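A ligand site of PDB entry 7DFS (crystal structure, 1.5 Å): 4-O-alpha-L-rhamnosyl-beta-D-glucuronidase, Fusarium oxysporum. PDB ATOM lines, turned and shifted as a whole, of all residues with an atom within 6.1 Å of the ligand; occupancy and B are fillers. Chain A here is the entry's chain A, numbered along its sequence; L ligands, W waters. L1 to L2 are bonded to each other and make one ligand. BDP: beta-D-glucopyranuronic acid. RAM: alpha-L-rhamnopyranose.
Merely in contact with the ligand: Gly 308 (3.3 Å), Thr 272 (3.5 Å), Phe 31 (3.5 Å), Ala 90 (3.6 Å), Gly 64 (3.7 Å), Tyr 224 (3.7 Å), Phe 195 (3.8 Å), Thr 66 (3.9 Å), Asn 312 (3.9 Å) and His 306 (3.9 Å).
Hydrophobic or aromatic side chains that line the ligand: Phe 31, Ala 90, Phe 195, Tyr 224 and Tyr 315.
Within 4 Å of the ligand: Glu 29, Phe 31, Gly 64, Thr 65, Thr 66, Ala 90, Asn 146, Glu 147, Phe 195, Tyr 224, Glu 267, Thr 272, Gln 273, Gly 274, His 306, Gly 308, Thr 309, Asn 312 and Tyr 315.
N of Gln 273 lies within hydrogen-bond range of O6B of BDP L1, at 2.6 Å.
The side-chain carboxylate of Glu 147 is in hydrogen-bond range of an oxygen (O1) of BDP L1 (2.6 Å).
An oxygen (O3) of BDP L1 lies within hydrogen-bond range of the side-chain carboxylate (OE1) of Glu 29, at 2.6 Å.
The backbone NH (N) of Gly 274 is in hydrogen-bond range of an oxygen (O6A) of BDP L1, 2.7 Å away.
The side-chain hydroxyl of Tyr 315 sits at hydrogen-bond distance from an oxygen (O6A) of BDP L1, 2.7 Å away.
An oxygen (O3) of RAM L2 sits at hydrogen-bond distance from the backbone NH of Thr 309.
An oxygen (O4) of RAM L2 sits at hydrogen-bond distance from the side-chain hydroxyl (OG1) of Thr 309, 2.7 Å away.
N of Thr 65 lies within hydrogen-bond range of O3 of BDP L1 (2.9 Å).
The side-chain hydroxyl of Thr 65 is in hydrogen-bond range of an oxygen (O3) of BDP L1 (3.2 Å).
The side-chain carboxylate (OE1) of Glu 267 is in hydrogen-bond range of an oxygen (O2) of BDP L1 (3.0 Å).
An oxygen (O2) of BDP L1 is in hydrogen-bond range of the side-chain amide nitrogen of Asn 146.
Water W5 lies within hydrogen-bond range of O3 of RAM L2, SG of Cys 313, OH of Tyr 315 and O of Gly 274.
Water W2 lies within hydrogen-bond range of O of Asn 312 (2.7 Å) and O3 of RAM L2 (2.8 Å).
Water W1 lies within hydrogen-bond range of O of Gln 273 (2.7 Å) and O2 of RAM L2 (3.4 Å).
The side-chain amide nitrogen (NE2) of Gln 273 sits at hydrogen-bond distance from the backbone carbonyl oxygen (O) of Gly 275 (2.5 Å).
A ring nitrogen (ND1) of His 222 is in hydrogen-bond range of the side-chain carboxylate (OE2) of Glu 147 (2.6 Å).
The side-chain carboxylate (OE2) of Glu 29 is in hydrogen-bond range of the backbone NH (N) of Thr 65.
The side-chain carboxylate (OE1) of Glu 29 sits at hydrogen-bond distance from a ring nitrogen (NE2) of His 306 (2.8 Å).
N of Tyr 315 sits at hydrogen-bond distance from O of Gly 274.
OE2 of Glu 267 is in hydrogen-bond range of OH of Tyr 224, at 2.6 Å.
The side-chain amide oxygen (OD1) of Asn 146 is in hydrogen-bond range of the guanidinium group (NH2) of Arg 61.
The backbone NH (N) of Phe 31 lies within hydrogen-bond range of the side-chain hydroxyl (OG1) of Thr 66 (3.1 Å).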
ATOM      1  N   GLU A  29      -1.895 -27.861 -27.031  1.00  0.00           N
ATOM      2  CA  GLU A  29      -1.661 -26.422 -27.202  1.00  0.00           C
ATOM      3  C   GLU A  29      -2.965 -25.666 -26.833  1.00  0.00           C
ATOM      4  O   GLU A  29      -4.052 -25.995 -27.327  1.00  0.00           O
ATOM      5  CB  GLU A  29      -1.279 -26.138 -28.644  1.00  0.00           C
ATOM      6  CG  GLU A  29      -0.976 -24.664 -28.854  1.00  0.00           C
ATOM      7  CD  GLU A  29       0.267 -24.154 -28.143  1.00  0.00           C
ATOM      8  OE1 GLU A  29       1.309 -24.873 -28.123  1.00  0.00           O
ATOM      9  OE2 GLU A  29       0.205 -22.990 -27.637  1.00  0.00           O
ATOM     10  N   PHE A  31      -4.747 -22.906 -27.418  1.00  0.00           N
ATOM     11  CA  PHE A  31      -5.855 -22.420 -28.320  1.00  0.00           C
ATOM     12  C   PHE A  31      -6.562 -23.588 -28.989  1.00  0.00           C
ATOM     13  O   PHE A  31      -7.737 -23.402 -29.367  1.00  0.00           O
ATOM     14  CB  PHE A  31      -5.326 -21.453 -29.376  1.00  0.00           C
ATOM     15  CG  PHE A  31      -4.728 -22.114 -30.585  1.00  0.00           C
ATOM     16  CD1 PHE A  31      -3.413 -22.556 -30.595  1.00  0.00           C
ATOM     17  CD2 PHE A  31      -5.502 -22.318 -31.715  1.00  0.00           C
ATOM     18  CE1 PHE A  31      -2.880 -23.147 -31.730  1.00  0.00           C
ATOM     19  CE2 PHE A  31      -4.978 -22.932 -32.844  1.00  0.00           C
ATOM     20  CZ  PHE A  31      -3.669 -23.333 -32.844  1.00  0.00           C
ATOM     21  N   ALA A  32      -5.869 -24.729 -29.176  1.00  0.00           N
ATOM     22  CA  ALA A  32      -6.345 -25.901 -29.941  1.00  0.00           C
ATOM     23  C   ALA A  32      -7.090 -26.879 -29.066  1.00  0.00           C
ATOM     24  O   ALA A  32      -7.687 -27.817 -29.593  1.00  0.00           O
ATOM     25  CB  ALA A  32      -5.170 -26.561 -30.612  1.00  0.00           C
ATOM     26  N   ARG A  61      -2.548 -31.771 -19.799  1.00  0.00           N
ATOM     27  CA  ARG A  61      -2.138 -30.384 -19.585  1.00  0.00           C
ATOM     28  C   ARG A  61      -2.555 -29.572 -20.806  1.00  0.00           C
ATOM     29  O   ARG A  61      -2.475 -30.079 -21.920  1.00  0.00           O
ATOM     30  CB  ARG A  61      -0.622 -30.346 -19.353  1.00  0.00           C
ATOM     31  CG  ARG A  61      -0.103 -28.937 -19.190  1.00  0.00           C
ATOM     32  CD  ARG A  61       0.434 -28.400 -20.513  1.00  0.00           C
ATOM     33  NE  ARG A  61       1.027 -27.063 -20.310  1.00  0.00           N
ATOM     34  CZ  ARG A  61       1.820 -26.493 -21.195  1.00  0.00           C
ATOM     35  NH1 ARG A  61       2.012 -27.037 -22.378  1.00  0.00           N
ATOM     36  NH2 ARG A  61       2.350 -25.328 -20.913  1.00  0.00           N
ATOM     37  N   GLY A  63      -1.881 -25.947 -22.470  1.00  0.00           N
ATOM     38  CA  GLY A  63      -0.962 -24.835 -22.344  1.00  0.00           C
ATOM     39  C   GLY A  63      -0.057 -24.755 -23.560  1.00  0.00           C
ATOM     40  O   GLY A  63      -0.337 -25.391 -24.594  1.00  0.00           O
ATOM     41  N   GLY A  64       0.967 -23.921 -23.469  1.00  0.00           N
ATOM     42  CA  GLY A  64       1.909 -23.682 -24.579  1.00  0.00           C
ATOM     43  C   GLY A  64       2.030 -22.183 -24.826  1.00  0.00           C
ATOM     44  O   GLY A  64       1.515 -21.342 -24.061  1.00  0.00           O
ATOM     45  N   THR A  65       2.787 -21.818 -25.839  1.00  0.00           N
ATOM     46  CA  THR A  65       3.013 -20.393 -26.169  1.00  0.00           C
ATOM     47  C   THR A  65       1.690 -19.641 -26.224  1.00  0.00           C
ATOM     48  O   THR A  65       1.620 -18.474 -25.809  1.00  0.00           O
ATOM     49  CB  THR A  65       3.776 -20.240 -27.477  1.00  0.00           C
ATOM     50  OG1 THR A  65       5.033 -20.880 -27.230  1.00  0.00           O
ATOM     51  CG2 THR A  65       4.047 -18.793 -27.828  1.00  0.00           C
ATOM     52  N   THR A  66       0.659 -20.238 -26.810  1.00  0.00           N
ATOM     53  CA  THR A  66      -0.633 -19.519 -26.967  1.00  0.00           C
ATOM     54  C   THR A  66      -1.309 -19.214 -25.615  1.00  0.00           C
ATOM     55  O   THR A  66      -2.199 -18.333 -25.592  1.00  0.00           O
ATOM     56  CB  THR A  66      -1.580 -20.177 -27.968  1.00  0.00           C
ATOM     57  OG1 THR A  66      -1.973 -21.490 -27.569  1.00  0.00           O
ATOM     58  CG2 THR A  66      -0.960 -20.211 -29.346  1.00  0.00           C
ATOM     59  N   ARG A  69      -0.826 -15.796 -25.062  1.00  0.00           N
ATOM     60  CA  ARG A  69      -1.438 -14.906 -26.085  1.00  0.00           C
ATOM     61  C   ARG A  69      -2.925 -14.735 -25.776  1.00  0.00           C
ATOM     62  O   ARG A  69      -3.651 -14.101 -26.592  1.00  0.00           O
ATOM     63  CB  ARG A  69      -1.278 -15.472 -27.503  1.00  0.00           C
ATOM     64  CG  ARG A  69       0.179 -15.657 -27.877  1.00  0.00           C
ATOM     65  CD  ARG A  69       0.301 -16.134 -29.283  1.00  0.00           C
ATOM     66  NE  ARG A  69       1.678 -16.358 -29.686  1.00  0.00           N
ATOM     67  CZ  ARG A  69       2.028 -17.005 -30.787  1.00  0.00           C
ATOM     68  NH1 ARG A  69       1.127 -17.487 -31.618  1.00  0.00           N
ATOM     69  NH2 ARG A  69       3.297 -17.225 -31.066  1.00  0.00           N
ATOM     70  N   ALA A  90      -1.133 -20.663 -35.886  1.00  0.00           N
ATOM     71  CA  ALA A  90      -1.635 -20.430 -34.516  1.00  0.00           C
ATOM     72  C   ALA A  90      -2.006 -18.964 -34.420  1.00  0.00           C
ATOM     73  O   ALA A  90      -1.352 -18.090 -35.014  1.00  0.00           O
ATOM     74  CB  ALA A  90      -0.591 -20.867 -33.514  1.00  0.00           C
ATOM     75  N   ASN A 146       3.904 -19.713 -19.456  1.00  0.00           N
ATOM     76  CA  ASN A 146       4.586 -20.813 -20.193  1.00  0.00           C
ATOM     77  C   ASN A 146       5.981 -20.360 -20.608  1.00  0.00           C
ATOM     78  O   ASN A 146       6.092 -19.320 -21.210  1.00  0.00           O
ATOM     79  CB  ASN A 146       3.722 -21.189 -21.398  1.00  0.00           C
ATOM     80  CG  ASN A 146       4.358 -22.214 -22.305  1.00  0.00           C
ATOM     81  OD1 ASN A 146       4.293 -23.428 -22.034  1.00  0.00           O
ATOM     82  ND2 ASN A 146       4.936 -21.755 -23.420  1.00  0.00           N
ATOM     83  N   GLU A 147       7.015 -21.127 -20.295  1.00  0.00           N
ATOM     84  CA  GLU A 147       8.394 -20.837 -20.816  1.00  0.00           C
ATOM     85  C   GLU A 147       8.746 -19.371 -20.609  1.00  0.00           C
ATOM     86  O   GLU A 147       9.114 -18.666 -21.559  1.00  0.00           O
ATOM     87  CB  GLU A 147       8.492 -21.245 -22.275  1.00  0.00           C
ATOM     88  CG  GLU A 147       8.250 -22.759 -22.411  1.00  0.00           C
ATOM     89  CD  GLU A 147       8.399 -23.333 -23.804  1.00  0.00           C
ATOM     90  OE1 GLU A 147       8.632 -22.546 -24.761  1.00  0.00           O
ATOM     91  OE2 GLU A 147       8.310 -24.579 -23.944  1.00  0.00           O
ATOM     92  N   PHE A 150      11.630 -17.397 -22.248  1.00  0.00           N
ATOM     93  CA  PHE A 150      11.597 -16.772 -23.590  1.00  0.00           C
ATOM     94  C   PHE A 150      10.923 -15.401 -23.555  1.00  0.00           C
ATOM     95  O   PHE A 150      10.841 -14.767 -24.643  1.00  0.00           O
ATOM     96  CB  PHE A 150      10.909 -17.680 -24.600  1.00  0.00           C
ATOM     97  CG  PHE A 150      11.649 -18.941 -24.948  1.00  0.00           C
ATOM     98  CD1 PHE A 150      13.013 -18.933 -25.212  1.00  0.00           C
ATOM     99  CD2 PHE A 150      10.978 -20.156 -25.034  1.00  0.00           C
ATOM    100  CE1 PHE A 150      13.671 -20.090 -25.594  1.00  0.00           C
ATOM    101  CE2 PHE A 150      11.654 -21.319 -25.354  1.00  0.00           C
ATOM    102  CZ  PHE A 150      13.003 -21.294 -25.627  1.00  0.00           C
ATOM    103  N   PHE A 195      11.670 -23.782 -20.477  1.00  0.00           N
ATOM    104  CA  PHE A 195      12.307 -24.549 -21.575  1.00  0.00           C
ATOM    105  C   PHE A 195      13.760 -24.810 -21.216  1.00  0.00           C
ATOM    106  O   PHE A 195      14.530 -23.870 -21.055  1.00  0.00           O
ATOM    107  CB  PHE A 195      12.170 -23.822 -22.905  1.00  0.00           C
ATOM    108  CG  PHE A 195      12.597 -24.622 -24.125  1.00  0.00           C
ATOM    109  CD1 PHE A 195      13.923 -24.654 -24.522  1.00  0.00           C
ATOM    110  CD2 PHE A 195      11.629 -25.243 -24.932  1.00  0.00           C
ATOM    111  CE1 PHE A 195      14.302 -25.340 -25.678  1.00  0.00           C
ATOM    112  CE2 PHE A 195      12.007 -25.916 -26.093  1.00  0.00           C
ATOM    113  CZ  PHE A 195      13.347 -25.994 -26.434  1.00  0.00           C
ATOM    114  N   HIS A 222      10.133 -28.027 -19.392  1.00  0.00           N
ATOM    115  CA  HIS A 222       9.894 -28.418 -20.795  1.00  0.00           C
ATOM    116  C   HIS A 222      11.177 -28.959 -21.401  1.00  0.00           C
ATOM    117  O   HIS A 222      12.266 -28.469 -21.071  1.00  0.00           O
ATOM    118  CB  HIS A 222       9.345 -27.226 -21.562  1.00  0.00           C
ATOM    119  CG  HIS A 222       7.960 -26.820 -21.177  1.00  0.00           C
ATOM    120  ND1 HIS A 222       7.259 -25.895 -21.915  1.00  0.00           N
ATOM    121  CD2 HIS A 222       7.156 -27.226 -20.148  1.00  0.00           C
ATOM    122  CE1 HIS A 222       6.070 -25.738 -21.342  1.00  0.00           C
ATOM    123  NE2 HIS A 222       5.992 -26.547 -20.288  1.00  0.00           N
ATOM    124  N   TYR A 224      12.585 -30.457 -25.316  1.00  0.00           N
ATOM    125  CA  TYR A 224      12.512 -30.827 -26.739  1.00  0.00           C
ATOM    126  C   TYR A 224      13.952 -31.081 -27.149  1.00  0.00           C
ATOM    127  O   TYR A 224      14.739 -30.148 -27.286  1.00  0.00           O
ATOM    128  CB  TYR A 224      11.899 -29.718 -27.598  1.00  0.00           C
ATOM    129  CG  TYR A 224      10.411 -29.578 -27.459  1.00  0.00           C
ATOM    130  CD1 TYR A 224       9.839 -28.901 -26.386  1.00  0.00           C
ATOM    131  CD2 TYR A 224       9.554 -30.037 -28.456  1.00  0.00           C
ATOM    132  CE1 TYR A 224       8.455 -28.713 -26.308  1.00  0.00           C
ATOM    133  CE2 TYR A 224       8.193 -29.875 -28.377  1.00  0.00           C
ATOM    134  CZ  TYR A 224       7.625 -29.224 -27.294  1.00  0.00           C
ATOM    135  OH  TYR A 224       6.277 -29.017 -27.283  1.00  0.00           O
ATOM    136  N   GLU A 267       5.591 -30.265 -20.613  1.00  0.00           N
ATOM    137  CA  GLU A 267       5.428 -30.160 -22.068  1.00  0.00           C
ATOM    138  C   GLU A 267       6.698 -30.697 -22.678  1.00  0.00           C
ATOM    139  O   GLU A 267       7.764 -30.182 -22.374  1.00  0.00           O
ATOM    140  CB  GLU A 267       5.143 -28.743 -22.502  1.00  0.00           C
ATOM    141  CG  GLU A 267       4.769 -28.674 -23.962  1.00  0.00           C
ATOM    142  CD  GLU A 267       4.806 -27.284 -24.532  1.00  0.00           C
ATOM    143  OE1 GLU A 267       4.179 -26.381 -23.986  1.00  0.00           O
ATOM    144  OE2 GLU A 267       5.430 -27.149 -25.618  1.00  0.00           O
ATOM    145  N   ALA A 271      10.874 -32.576 -31.218  1.00  0.00           N
ATOM    146  CA  ALA A 271      11.529 -31.420 -31.811  1.00  0.00           C
ATOM    147  C   ALA A 271      10.592 -30.243 -31.939  1.00  0.00           C
ATOM    148  O   ALA A 271       9.432 -30.422 -32.113  1.00  0.00           O
ATOM    149  CB  ALA A 271      12.089 -31.808 -33.174  1.00  0.00           C
ATOM    150  N   THR A 272      11.146 -29.044 -31.867  1.00  0.00           N
ATOM    151  CA  THR A 272      10.402 -27.805 -31.935  1.00  0.00           C
ATOM    152  C   THR A 272       9.905 -27.380 -33.302  1.00  0.00           C
ATOM    153  O   THR A 272      10.306 -27.924 -34.246  1.00  0.00           O
ATOM    154  CB  THR A 272      11.146 -26.660 -31.281  1.00  0.00           C
ATOM    155  OG1 THR A 272      12.451 -26.579 -31.819  1.00  0.00           O
ATOM    156  CG2 THR A 272      11.254 -26.895 -29.802  1.00  0.00           C
ATOM    157  N   GLN A 273       9.137 -26.301 -33.255  1.00  0.00           N
ATOM    158  CA  GLN A 273       8.290 -25.605 -34.261  1.00  0.00           C
ATOM    159  C   GLN A 273       7.206 -26.570 -34.769  1.00  0.00           C
ATOM    160  O   GLN A 273       6.731 -26.405 -35.898  1.00  0.00           O
ATOM    161  CB  GLN A 273       9.199 -24.974 -35.327  1.00  0.00           C
ATOM    162  CG  GLN A 273      10.285 -25.879 -35.857  1.00  0.00           C
ATOM    163  CD  GLN A 273       9.767 -26.929 -36.833  1.00  0.00           C
ATOM    164  OE1 GLN A 273      10.209 -26.990 -37.975  1.00  0.00           O
ATOM    165  NE2 GLN A 273       8.854 -27.780 -36.373  1.00  0.00           N
ATOM    166  N   GLY A 274       6.791 -27.533 -33.919  1.00  0.00           N
ATOM    167  CA  GLY A 274       5.731 -28.469 -34.233  1.00  0.00           C
ATOM    168  C   GLY A 274       6.312 -29.801 -34.662  1.00  0.00           C
ATOM    169  O   GLY A 274       5.537 -30.712 -34.951  1.00  0.00           O
ATOM    170  N   GLY A 275       7.644 -29.872 -34.709  1.00  0.00           N
ATOM    171  CA  GLY A 275       8.367 -31.074 -35.117  1.00  0.00           C
ATOM    172  C   GLY A 275       8.985 -30.944 -36.525  1.00  0.00           C
ATOM    173  O   GLY A 275       8.575 -30.120 -37.277  1.00  0.00           O
ATOM    174  N   HIS A 306       3.443 -33.023 -26.123  1.00  0.00           N
ATOM    175  CA  HIS A 306       2.698 -31.892 -26.696  1.00  0.00           C
ATOM    176  C   HIS A 306       2.031 -32.257 -28.023  1.00  0.00           C
ATOM    177  O   HIS A 306       2.643 -32.965 -28.866  1.00  0.00           O
ATOM    178  CB  HIS A 306       3.624 -30.714 -26.913  1.00  0.00           C
ATOM    179  CG  HIS A 306       2.872 -29.423 -27.000  1.00  0.00           C
ATOM    180  ND1 HIS A 306       2.024 -29.015 -25.975  1.00  0.00           N
ATOM    181  CD2 HIS A 306       2.863 -28.439 -27.933  1.00  0.00           C
ATOM    182  CE1 HIS A 306       1.533 -27.837 -26.283  1.00  0.00           C
ATOM    183  NE2 HIS A 306       2.049 -27.441 -27.459  1.00  0.00           N
ATOM    184  N   HIS A 307       0.843 -31.715 -28.191  1.00  0.00           N
ATOM    185  CA  HIS A 307      -0.020 -31.831 -29.394  1.00  0.00           C
ATOM    186  C   HIS A 307      -0.352 -30.424 -29.835  1.00  0.00           C
ATOM    187  O   HIS A 307      -0.944 -29.679 -29.068  1.00  0.00           O
ATOM    188  CB  HIS A 307      -1.241 -32.676 -29.029  1.00  0.00           C
ATOM    189  CG  HIS A 307      -0.903 -34.120 -29.027  1.00  0.00           C
ATOM    190  ND1 HIS A 307      -0.055 -34.690 -28.069  1.00  0.00           N
ATOM    191  CD2 HIS A 307      -1.208 -35.098 -29.923  1.00  0.00           C
ATOM    192  CE1 HIS A 307       0.126 -35.973 -28.434  1.00  0.00           C
ATOM    193  NE2 HIS A 307      -0.559 -36.238 -29.562  1.00  0.00           N
ATOM    194  N   GLY A 308       0.132 -30.057 -31.034  1.00  0.00           N
ATOM    195  CA  GLY A 308       0.032 -28.651 -31.498  1.00  0.00           C
ATOM    196  C   GLY A 308      -1.118 -28.446 -32.441  1.00  0.00           C
ATOM    197  O   GLY A 308      -2.134 -29.138 -32.397  1.00  0.00           O
ATOM    198  N   THR A 309      -0.959 -27.469 -33.322  1.00  0.00           N
ATOM    199  CA  THR A 309      -2.024 -27.046 -34.250  1.00  0.00           C
ATOM    200  C   THR A 309      -2.571 -28.203 -35.048  1.00  0.00           C
ATOM    201  O   THR A 309      -1.802 -28.951 -35.694  1.00  0.00           O
ATOM    202  CB  THR A 309      -1.465 -26.010 -35.216  1.00  0.00           C
ATOM    203  OG1 THR A 309      -0.977 -24.927 -34.450  1.00  0.00           O
ATOM    204  CG2 THR A 309      -2.515 -25.508 -36.185  1.00  0.00           C
ATOM    205  N   ASN A 312      -1.389 -29.246 -38.573  1.00  0.00           N
ATOM    206  CA  ASN A 312      -0.008 -28.743 -38.803  1.00  0.00           C
ATOM    207  C   ASN A 312       0.851 -29.124 -37.581  1.00  0.00           C
ATOM    208  O   ASN A 312       1.381 -28.260 -36.914  1.00  0.00           O
ATOM    209  CB  ASN A 312      -0.007 -27.260 -39.121  1.00  0.00           C
ATOM    210  CG  ASN A 312       1.346 -26.738 -39.556  1.00  0.00           C
ATOM    211  OD1 ASN A 312       2.243 -27.529 -39.899  1.00  0.00           O
ATOM    212  ND2 ASN A 312       1.509 -25.437 -39.592  1.00  0.00           N
ATOM    213  N   CYS A 313       0.983 -30.408 -37.361  1.00  0.00           N
ATOM    214  CA  CYS A 313       1.646 -30.941 -36.157  1.00  0.00           C
ATOM    215  C   CYS A 313       2.388 -32.237 -36.475  1.00  0.00           C
ATOM    216  O   CYS A 313       1.735 -33.258 -36.789  1.00  0.00           O
ATOM    217  CB  CYS A 313       0.590 -31.204 -35.102  1.00  0.00           C
ATOM    218  SG  CYS A 313       1.369 -31.853 -33.599  1.00  0.00           S
ATOM    219  N   TYR A 315       4.648 -33.893 -34.499  1.00  0.00           N
ATOM    220  CA  TYR A 315       4.942 -34.783 -33.354  1.00  0.00           C
ATOM    221  C   TYR A 315       3.668 -35.296 -32.699  1.00  0.00           C
ATOM    222  O   TYR A 315       3.773 -36.075 -31.750  1.00  0.00           O
ATOM    223  CB  TYR A 315       5.854 -34.116 -32.333  1.00  0.00           C
ATOM    224  CG  TYR A 315       5.567 -32.715 -31.911  1.00  0.00           C
ATOM    225  CD1 TYR A 315       4.308 -32.342 -31.444  1.00  0.00           C
ATOM    226  CD2 TYR A 315       6.549 -31.740 -31.938  1.00  0.00           C
ATOM    227  CE1 TYR A 315       4.027 -31.059 -31.057  1.00  0.00           C
ATOM    228  CE2 TYR A 315       6.297 -30.446 -31.511  1.00  0.00           C
ATOM    229  CZ  TYR A 315       5.027 -30.106 -31.066  1.00  0.00           C
ATOM    230  OH  TYR A 315       4.701 -28.848 -30.706  1.00  0.00           O
HETATM  231  C1  BDP L   1       7.126 -25.130 -27.180  1.00  0.00           C
HETATM  232  C2  BDP L   1       5.893 -24.212 -26.923  1.00  0.00           C
HETATM  233  C3  BDP L   1       4.798 -24.682 -27.863  1.00  0.00           C
HETATM  234  C4  BDP L   1       5.369 -24.836 -29.276  1.00  0.00           C
HETATM  235  C5  BDP L   1       6.523 -25.871 -29.276  1.00  0.00           C
HETATM  236  C6  BDP L   1       7.101 -26.212 -30.601  1.00  0.00           C
HETATM  237  O2  BDP L   1       5.411 -24.145 -25.556  1.00  0.00           O
HETATM  238  O3  BDP L   1       3.692 -23.765 -27.832  1.00  0.00           O
HETATM  239  O4  BDP L   1       4.364 -25.312 -30.212  1.00  0.00           O
HETATM  240  O5  BDP L   1       7.539 -25.233 -28.508  1.00  0.00           O
HETATM  241  O6A BDP L   1       6.771 -27.201 -31.263  1.00  0.00           O
HETATM  242  O1  BDP L   1       8.293 -24.637 -26.586  1.00  0.00           O
HETATM  243  O6B BDP L   1       7.937 -25.385 -31.133  1.00  0.00           O
HETATM  244  C1  RAM L   2       4.467 -24.743 -31.499  1.00  0.00           C
HETATM  245  C2  RAM L   2       3.919 -25.707 -32.517  1.00  0.00           C
HETATM  246  C3  RAM L   2       2.374 -25.752 -32.379  1.00  0.00           C
HETATM  247  C4  RAM L   2       1.749 -24.363 -32.358  1.00  0.00           C
HETATM  248  C5  RAM L   2       2.401 -23.551 -31.281  1.00  0.00           C
HETATM  249  C6  RAM L   2       1.856 -22.144 -31.229  1.00  0.00           C
HETATM  250  O2  RAM L   2       4.202 -25.141 -33.769  1.00  0.00           O
HETATM  251  O3  RAM L   2       1.809 -26.565 -33.413  1.00  0.00           O
HETATM  252  O4  RAM L   2       0.318 -24.509 -32.070  1.00  0.00           O
HETATM  253  O5  RAM L   2       3.815 -23.446 -31.510  1.00  0.00           O
HETATM  254  O   HOH W   1       4.666 -25.201 -37.135  1.00  0.00           O
HETATM  255  O   HOH W   2       2.356 -25.890 -36.076  1.00  0.00           O
HETATM  256  O   HOH W   3      10.338 -23.229 -28.393  1.00  0.00           O
HETATM  257  O   HOH W   4       4.294 -22.400 -34.397  1.00  0.00           O
HETATM  258  O   HOH W   5       3.018 -29.019 -33.570  1.00  0.00           O
